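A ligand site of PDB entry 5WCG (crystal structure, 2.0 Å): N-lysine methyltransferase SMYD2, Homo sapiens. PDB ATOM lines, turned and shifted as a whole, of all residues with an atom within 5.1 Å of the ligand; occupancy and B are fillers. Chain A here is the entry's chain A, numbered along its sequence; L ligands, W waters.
A nitrogen (N3) of the ligand lies within hydrogen-bond range of the backbone NH (N) of His 207. N6 of the ligand lies within hydrogen-bond range of O of His 207 (3.0 Å). NE2 of His 137 lies within hydrogen-bond range of O1 of the ligand, at 3.1 Å.
The backbone NH of Tyr 240 is in hydrogen-bond range of a ring nitrogen (ND1) of His 207, 3.0 Å away. A ring nitrogen (NE2) of His 137 is in hydrogen-bond range of the backbone carbonyl oxygen (O) of Tyr 258 (3.3 Å). SG of Cys 181 lies within hydrogen-bond range of ND2 of Asn 182, at 3.5 Å. SG of Cys 181 sits at hydrogen-bond distance from O of Glu 135 (3.3 Å). O of Glu 135 lies within hydrogen-bond range of ND2 of Asn 182 (2.9 Å).
A nitrogen (N4) of the ligand sits close to the side-chain amide oxygen (OD1) of Asn 206 (3.3 Å). The backbone carbonyl oxygen of Tyr 258 sits close to an oxygen (O1) of the ligand (3.3 Å). Gly 16 touches the ligand. Lys 17 touches the ligand (O to C3, 3.7 Å). SG of Cys 181 touches C7 of the ligand, 3.4 Å away. O of Asn 182 touches C20 of the ligand, 3.5 Å away. O of Gly 183 touches C26 of the ligand, 3.5 Å away. Phe 184 touches the ligand. Ala 203 touches the ligand (O to C9, 3.5 Å). Tyr 240 touches the ligand. Phe 260 touches the ligand. Hydrophobic or aromatic side chains within 4 Å of the ligand: His 137, Phe 184, Ala 203, His 207, Tyr 240, Tyr 258 and Phe 260. 13 residues have an atom within 4 Å of the ligand: Gly 16, Lys 17, His 137, Cys 181, Asn 182, Gly 183, Phe 184, Ala 203, Asn 206, His 207, Tyr 240, Tyr 258 and Phe 260.
Water W2 lies within hydrogen-bond range of a nitrogen (N1) of the ligand (2.7 Å), the backbone carbonyl oxygen (O) of Thr 261 (3.0 Å) and the backbone NH (N) of Glu 263 (3.3 Å). Water W8 bridges O of Tyr 258 (2.6 Å) and O1 of the ligand (2.8 Å). Water W1 bridges N2 of the ligand (2.8 Å) and O of Lys 17 (3.0 Å). Water W7 lies within hydrogen-bond range of a nitrogen (N6) of the ligand (2.9 Å) and the backbone NH (N) of Glu 263 (3.1 Å). Water W5 lies within hydrogen-bond range of the side-chain amide oxygen of Asn 206 (2.8 Å) and the backbone carbonyl oxygen of Lys 17 (3.5 Å). Water W6 bridges O of His 207 (3.0 Å) and N6 of the ligand (3.5 Å).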
ATOM      1  N   GLY A  16      21.081  34.919 -16.606  1.00  0.00           N
ATOM      2  CA  GLY A  16      20.453  34.135 -15.573  1.00  0.00           C
ATOM      3  C   GLY A  16      19.323  33.222 -16.044  1.00  0.00           C
ATOM      4  O   GLY A  16      18.841  32.412 -15.254  1.00  0.00           O
ATOM      5  N   LYS A  17      18.907  33.331 -17.309  1.00  0.00           N
ATOM      6  CA  LYS A  17      17.716  32.631 -17.824  1.00  0.00           C
ATOM      7  C   LYS A  17      17.976  31.761 -19.043  1.00  0.00           C
ATOM      8  O   LYS A  17      17.486  30.654 -19.109  1.00  0.00           O
ATOM      9  CB  LYS A  17      16.617  33.640 -18.160  1.00  0.00           C
ATOM     10  CG  LYS A  17      16.116  34.407 -16.955  1.00  0.00           C
ATOM     11  CD  LYS A  17      15.000  35.377 -17.306  1.00  0.00           C
ATOM     12  CE  LYS A  17      14.591  36.258 -16.148  1.00  0.00           C
ATOM     13  NZ  LYS A  17      15.718  37.077 -15.610  1.00  0.00           N
ATOM     14  N   GLU A 135      13.372  22.439 -25.570  1.00  0.00           N
ATOM     15  CA  GLU A 135      13.725  21.787 -24.318  1.00  0.00           C
ATOM     16  C   GLU A 135      12.852  20.539 -24.124  1.00  0.00           C
ATOM     17  O   GLU A 135      11.642  20.573 -24.403  1.00  0.00           O
ATOM     18  CB  GLU A 135      13.499  22.730 -23.130  1.00  0.00           C
ATOM     19  CG  GLU A 135      14.414  23.943 -23.075  1.00  0.00           C
ATOM     20  CD  GLU A 135      15.857  23.587 -22.719  1.00  0.00           C
ATOM     21  OE1 GLU A 135      16.777  24.248 -23.252  1.00  0.00           O
ATOM     22  OE2 GLU A 135      16.071  22.640 -21.931  1.00  0.00           O
ATOM     23  N   HIS A 137      13.789  18.587 -21.060  1.00  0.00           N
ATOM     24  CA  HIS A 137      14.001  18.284 -19.642  1.00  0.00           C
ATOM     25  C   HIS A 137      14.082  16.783 -19.289  1.00  0.00           C
ATOM     26  O   HIS A 137      13.792  16.356 -18.149  1.00  0.00           O
ATOM     27  CB  HIS A 137      12.910  18.938 -18.796  1.00  0.00           C
ATOM     28  CG  HIS A 137      12.951  20.432 -18.864  1.00  0.00           C
ATOM     29  ND1 HIS A 137      11.943  21.190 -19.436  1.00  0.00           N
ATOM     30  CD2 HIS A 137      13.913  21.303 -18.497  1.00  0.00           C
ATOM     31  CE1 HIS A 137      12.274  22.461 -19.388  1.00  0.00           C
ATOM     32  NE2 HIS A 137      13.463  22.563 -18.810  1.00  0.00           N
ATOM     33  N   CYS A 181       6.011  19.508 -22.604  1.00  0.00           N
ATOM     34  CA  CYS A 181       6.333  20.791 -21.980  1.00  0.00           C
ATOM     35  C   CYS A 181       6.275  22.011 -22.896  1.00  0.00           C
ATOM     36  O   CYS A 181       6.180  23.129 -22.397  1.00  0.00           O
ATOM     37  CB  CYS A 181       7.669  20.702 -21.224  1.00  0.00           C
ATOM     38  SG  CYS A 181       9.095  20.493 -22.268  1.00  0.00           S
ATOM     39  N   ASN A 182       6.261  21.829 -24.213  1.00  0.00           N
ATOM     40  CA  ASN A 182       6.177  22.936 -25.183  1.00  0.00           C
ATOM     41  C   ASN A 182       4.808  23.165 -25.841  1.00  0.00           C
ATOM     42  O   ASN A 182       4.587  24.239 -26.429  1.00  0.00           O
ATOM     43  CB  ASN A 182       7.217  22.799 -26.305  1.00  0.00           C
ATOM     44  CG  ASN A 182       8.631  22.994 -25.813  1.00  0.00           C
ATOM     45  OD1 ASN A 182       9.111  24.119 -25.772  1.00  0.00           O
ATOM     46  ND2 ASN A 182       9.293  21.893 -25.417  1.00  0.00           N
ATOM     47  N   GLY A 183       3.934  22.176 -25.779  1.00  0.00           N
ATOM     48  CA  GLY A 183       2.632  22.273 -26.439  1.00  0.00           C
ATOM     49  C   GLY A 183       1.748  23.320 -25.790  1.00  0.00           C
ATOM     50  O   GLY A 183       1.763  23.480 -24.569  1.00  0.00           O
ATOM     51  N   PHE A 184       1.043  24.066 -26.624  1.00  0.00           N
ATOM     52  CA  PHE A 184       0.078  25.067 -26.192  1.00  0.00           C
ATOM     53  C   PHE A 184      -1.309  24.521 -26.354  1.00  0.00           C
ATOM     54  O   PHE A 184      -1.536  23.560 -27.120  1.00  0.00           O
ATOM     55  CB  PHE A 184       0.196  26.329 -27.071  1.00  0.00           C
ATOM     56  CG  PHE A 184       1.422  27.119 -26.797  1.00  0.00           C
ATOM     57  CD1 PHE A 184       2.604  26.823 -27.446  1.00  0.00           C
ATOM     58  CD2 PHE A 184       1.407  28.139 -25.859  1.00  0.00           C
ATOM     59  CE1 PHE A 184       3.751  27.547 -27.189  1.00  0.00           C
ATOM     60  CE2 PHE A 184       2.556  28.874 -25.594  1.00  0.00           C
ATOM     61  CZ  PHE A 184       3.728  28.584 -26.263  1.00  0.00           C
ATOM     62  N   THR A 185      -2.224  25.114 -25.602  1.00  0.00           N
ATOM     63  CA  THR A 185      -3.633  24.894 -25.771  1.00  0.00           C
ATOM     64  C   THR A 185      -4.176  26.098 -26.518  1.00  0.00           C
ATOM     65  O   THR A 185      -3.736  27.222 -26.280  1.00  0.00           O
ATOM     66  CB  THR A 185      -4.367  24.831 -24.441  1.00  0.00           C
ATOM     67  OG1 THR A 185      -3.845  23.753 -23.644  1.00  0.00           O
ATOM     68  CG2 THR A 185      -5.820  24.612 -24.702  1.00  0.00           C
ATOM     69  N   ALA A 203       7.369  29.855 -28.013  1.00  0.00           N
ATOM     70  CA  ALA A 203       8.087  29.103 -27.015  1.00  0.00           C
ATOM     71  C   ALA A 203       9.474  29.680 -26.676  1.00  0.00           C
ATOM     72  O   ALA A 203      10.146  29.187 -25.772  1.00  0.00           O
ATOM     73  CB  ALA A 203       8.209  27.647 -27.452  1.00  0.00           C
ATOM     74  N   ASN A 206      10.763  33.966 -22.417  1.00  0.00           N
ATOM     75  CA  ASN A 206      10.902  33.669 -21.011  1.00  0.00           C
ATOM     76  C   ASN A 206       9.662  34.079 -20.203  1.00  0.00           C
ATOM     77  O   ASN A 206       8.751  34.739 -20.709  1.00  0.00           O
ATOM     78  CB  ASN A 206      12.200  34.286 -20.469  1.00  0.00           C
ATOM     79  CG  ASN A 206      13.445  33.494 -20.930  1.00  0.00           C
ATOM     80  OD1 ASN A 206      13.425  32.247 -20.921  1.00  0.00           O
ATOM     81  ND2 ASN A 206      14.493  34.191 -21.351  1.00  0.00           N
ATOM     82  N   HIS A 207       9.650  33.631 -18.950  1.00  0.00           N
ATOM     83  CA  HIS A 207       8.507  33.806 -18.036  1.00  0.00           C
ATOM     84  C   HIS A 207       8.703  34.954 -17.061  1.00  0.00           C
ATOM     85  O   HIS A 207       9.782  35.121 -16.470  1.00  0.00           O
ATOM     86  CB  HIS A 207       8.287  32.530 -17.209  1.00  0.00           C
ATOM     87  CG  HIS A 207       7.406  32.725 -16.031  1.00  0.00           C
ATOM     88  ND1 HIS A 207       6.029  32.617 -16.118  1.00  0.00           N
ATOM     89  CD2 HIS A 207       7.677  33.120 -14.767  1.00  0.00           C
ATOM     90  CE1 HIS A 207       5.499  32.916 -14.935  1.00  0.00           C
ATOM     91  NE2 HIS A 207       6.481  33.236 -14.100  1.00  0.00           N
ATOM     92  N   SER A 239       3.652  34.764 -19.449  1.00  0.00           N
ATOM     93  CA  SER A 239       3.548  33.906 -18.274  1.00  0.00           C
ATOM     94  C   SER A 239       3.322  32.473 -18.713  1.00  0.00           C
ATOM     95  O   SER A 239       2.548  32.223 -19.616  1.00  0.00           O
ATOM     96  CB  SER A 239       2.384  34.341 -17.371  1.00  0.00           C
ATOM     97  OG  SER A 239       2.235  33.419 -16.307  1.00  0.00           O
ATOM     98  N   TYR A 240       4.020  31.547 -18.072  1.00  0.00           N
ATOM     99  CA  TYR A 240       3.844  30.119 -18.311  1.00  0.00           C
ATOM    100  C   TYR A 240       2.729  29.504 -17.471  1.00  0.00           C
ATOM    101  O   TYR A 240       2.309  28.384 -17.749  1.00  0.00           O
ATOM    102  CB  TYR A 240       5.129  29.361 -17.959  1.00  0.00           C
ATOM    103  CG  TYR A 240       6.386  29.699 -18.749  1.00  0.00           C
ATOM    104  CD1 TYR A 240       6.389  30.585 -19.828  1.00  0.00           C
ATOM    105  CD2 TYR A 240       7.609  29.064 -18.447  1.00  0.00           C
ATOM    106  CE1 TYR A 240       7.549  30.828 -20.547  1.00  0.00           C
ATOM    107  CE2 TYR A 240       8.764  29.297 -19.187  1.00  0.00           C
ATOM    108  CZ  TYR A 240       8.730  30.190 -20.214  1.00  0.00           C
ATOM    109  OH  TYR A 240       9.877  30.443 -20.944  1.00  0.00           O
ATOM    110  N   TYR A 258       8.944  22.855 -15.442  1.00  0.00           N
ATOM    111  CA  TYR A 258      10.087  23.435 -16.146  1.00  0.00           C
ATOM    112  C   TYR A 258      11.402  23.479 -15.390  1.00  0.00           C
ATOM    113  O   TYR A 258      12.391  23.900 -15.971  1.00  0.00           O
ATOM    114  CB  TYR A 258       9.755  24.853 -16.647  1.00  0.00           C
ATOM    115  CG  TYR A 258       8.396  24.946 -17.296  1.00  0.00           C
ATOM    116  CD1 TYR A 258       8.146  24.345 -18.514  1.00  0.00           C
ATOM    117  CD2 TYR A 258       7.341  25.601 -16.661  1.00  0.00           C
ATOM    118  CE1 TYR A 258       6.862  24.373 -19.075  1.00  0.00           C
ATOM    119  CE2 TYR A 258       6.057  25.629 -17.222  1.00  0.00           C
ATOM    120  CZ  TYR A 258       5.831  25.023 -18.439  1.00  0.00           C
ATOM    121  OH  TYR A 258       4.563  25.053 -18.981  1.00  0.00           O
ATOM    122  N   PHE A 260      12.592  25.275 -12.905  1.00  0.00           N
ATOM    123  CA  PHE A 260      13.185  26.540 -12.472  1.00  0.00           C
ATOM    124  C   PHE A 260      12.200  27.241 -11.587  1.00  0.00           C
ATOM    125  O   PHE A 260      11.021  26.871 -11.534  1.00  0.00           O
ATOM    126  CB  PHE A 260      13.600  27.443 -13.645  1.00  0.00           C
ATOM    127  CG  PHE A 260      12.447  28.136 -14.372  1.00  0.00           C
ATOM    128  CD1 PHE A 260      11.756  27.484 -15.397  1.00  0.00           C
ATOM    129  CD2 PHE A 260      12.079  29.445 -14.039  1.00  0.00           C
ATOM    130  CE1 PHE A 260      10.700  28.141 -16.076  1.00  0.00           C
ATOM    131  CE2 PHE A 260      11.010  30.076 -14.687  1.00  0.00           C
ATOM    132  CZ  PHE A 260      10.339  29.436 -15.709  1.00  0.00           C
ATOM    133  N   THR A 261      12.709  28.253 -10.872  1.00  0.00           N
ATOM    134  CA  THR A 261      11.884  29.140 -10.073  1.00  0.00           C
ATOM    135  C   THR A 261      12.108  30.582 -10.475  1.00  0.00           C
ATOM    136  O   THR A 261      13.195  30.975 -10.927  1.00  0.00           O
ATOM    137  CB  THR A 261      12.117  28.944  -8.564  1.00  0.00           C
ATOM    138  OG1 THR A 261      13.491  29.114  -8.269  1.00  0.00           O
ATOM    139  CG2 THR A 261      11.704  27.558  -8.096  1.00  0.00           C
ATOM    140  N   CYS A 262      11.057  31.369 -10.317  1.00  0.00           N
ATOM    141  CA  CYS A 262      10.991  32.715 -10.793  1.00  0.00           C
ATOM    142  C   CYS A 262      11.467  33.713  -9.717  1.00  0.00           C
ATOM    143  O   CYS A 262      11.187  33.552  -8.529  1.00  0.00           O
ATOM    144  CB  CYS A 262       9.538  33.038 -11.186  1.00  0.00           C
ATOM    145  SG  CYS A 262       9.361  34.625 -11.969  1.00  0.00           S
ATOM    146  N   GLU A 263      12.129  34.768 -10.193  1.00  0.00           N
ATOM    147  CA  GLU A 263      12.641  35.842  -9.350  1.00  0.00           C
ATOM    148  C   GLU A 263      12.080  37.183  -9.763  1.00  0.00           C
ATOM    149  O   GLU A 263      12.696  38.194  -9.500  1.00  0.00           O
ATOM    150  CB  GLU A 263      14.181  35.869  -9.413  1.00  0.00           C
ATOM    151  CG  GLU A 263      14.875  35.080  -8.326  1.00  0.00           C
ATOM    152  CD  GLU A 263      16.308  35.577  -8.156  1.00  0.00           C
ATOM    153  OE1 GLU A 263      17.063  35.516  -9.144  1.00  0.00           O
ATOM    154  OE2 GLU A 263      16.643  36.096  -7.064  1.00  0.00           O
HETATM  155  C1  LIG L   1      12.713  32.034 -16.720  1.00  0.00           C
HETATM  156  C2  LIG L   1      12.108  31.183 -18.555  1.00  0.00           C
HETATM  157  C3  LIG L   1      13.996  29.491 -18.950  1.00  0.00           C
HETATM  158  N1  LIG L   1      13.906  32.354 -14.668  1.00  0.00           N
HETATM  159  C4  LIG L   1      14.038  28.076 -18.321  1.00  0.00           C
HETATM  160  C5  LIG L   1      12.481  26.525 -19.489  1.00  0.00           C
HETATM  161  N2  LIG L   1      14.639  30.671 -16.212  1.00  0.00           N
HETATM  162  C6  LIG L   1      11.558  26.286 -20.584  1.00  0.00           C
HETATM  163  C7  LIG L   1       9.617  23.866 -22.215  1.00  0.00           C
HETATM  164  C8  LIG L   1      10.093  26.368 -22.219  1.00  0.00           C
HETATM  165  C9  LIG L   1       9.161  26.819 -23.318  1.00  0.00           C
HETATM  166  N3  LIG L   1      11.763  32.124 -17.718  1.00  0.00           N
HETATM  167  C10 LIG L   1       7.286  27.367 -21.860  1.00  0.00           C
HETATM  168  C11 LIG L   1       5.857  26.997 -21.492  1.00  0.00           C
HETATM  169  C12 LIG L   1       3.527  27.130 -22.362  1.00  0.00           C
HETATM  170  N4  LIG L   1      13.236  30.490 -18.186  1.00  0.00           N
HETATM  171  O1  LIG L   1      12.741  25.549 -18.750  1.00  0.00           O
HETATM  172  N5  LIG L   1      12.990  27.745 -19.287  1.00  0.00           N
HETATM  173  C13 LIG L   1      13.289  28.886 -20.171  1.00  0.00           C
HETATM  174  C14 LIG L   1      13.626  31.039 -16.987  1.00  0.00           C
HETATM  175  C15 LIG L   1      14.726  31.371 -15.067  1.00  0.00           C
HETATM  176  C16 LIG L   1      15.835  30.993 -14.124  1.00  0.00           C
HETATM  177  C17 LIG L   1      12.886  32.710 -15.500  1.00  0.00           C
HETATM  178  N6  LIG L   1      12.069  33.693 -15.088  1.00  0.00           N
HETATM  179  C18 LIG L   1      10.924  27.161 -21.482  1.00  0.00           C
HETATM  180  N7  LIG L   1      10.255  25.094 -21.780  1.00  0.00           N
HETATM  181  N8  LIG L   1      11.155  25.020 -20.776  1.00  0.00           N
HETATM  182  N9  LIG L   1       7.761  26.539 -22.977  1.00  0.00           N
HETATM  183  C19 LIG L   1       6.886  26.784 -24.133  1.00  0.00           C
HETATM  184  C20 LIG L   1       5.440  26.438 -23.795  1.00  0.00           C
HETATM  185  N10 LIG L   1       4.972  27.238 -22.638  1.00  0.00           N
HETATM  186  C21 LIG L   1       2.988  28.014 -21.205  1.00  0.00           C
HETATM  187  C22 LIG L   1       1.539  28.475 -21.327  1.00  0.00           C
HETATM  188  C23 LIG L   1       0.480  27.428 -21.011  1.00  0.00           C
HETATM  189  C24 LIG L   1       0.598  26.143 -21.839  1.00  0.00           C
HETATM  190  C25 LIG L   1       1.777  25.286 -21.537  1.00  0.00           C
HETATM  191  C26 LIG L   1       3.105  25.644 -22.197  1.00  0.00           C
HETATM  192  O   HOH W   1      16.710  28.905 -16.776  1.00  0.00           O
HETATM  193  O   HOH W   2      14.299  33.471 -12.265  1.00  0.00           O
HETATM  194  O   HOH W   3      16.525  28.458 -21.029  1.00  0.00           O
HETATM  195  O   HOH W   4       4.940  29.982 -23.188  1.00  0.00           O
HETATM  196  O   HOH W   5      15.439  30.514 -21.883  1.00  0.00           O
HETATM  197  O   HOH W   6      11.055  36.986 -14.563  1.00  0.00           O
HETATM  198  O   HOH W   7      12.691  35.724 -13.041  1.00  0.00           O
HETATM  199  O   HOH W   8      14.495  25.308 -16.624  1.00  0.00           O
HETATM  200  O   HOH W   9       2.548  22.017 -22.494  1.00  0.00           O
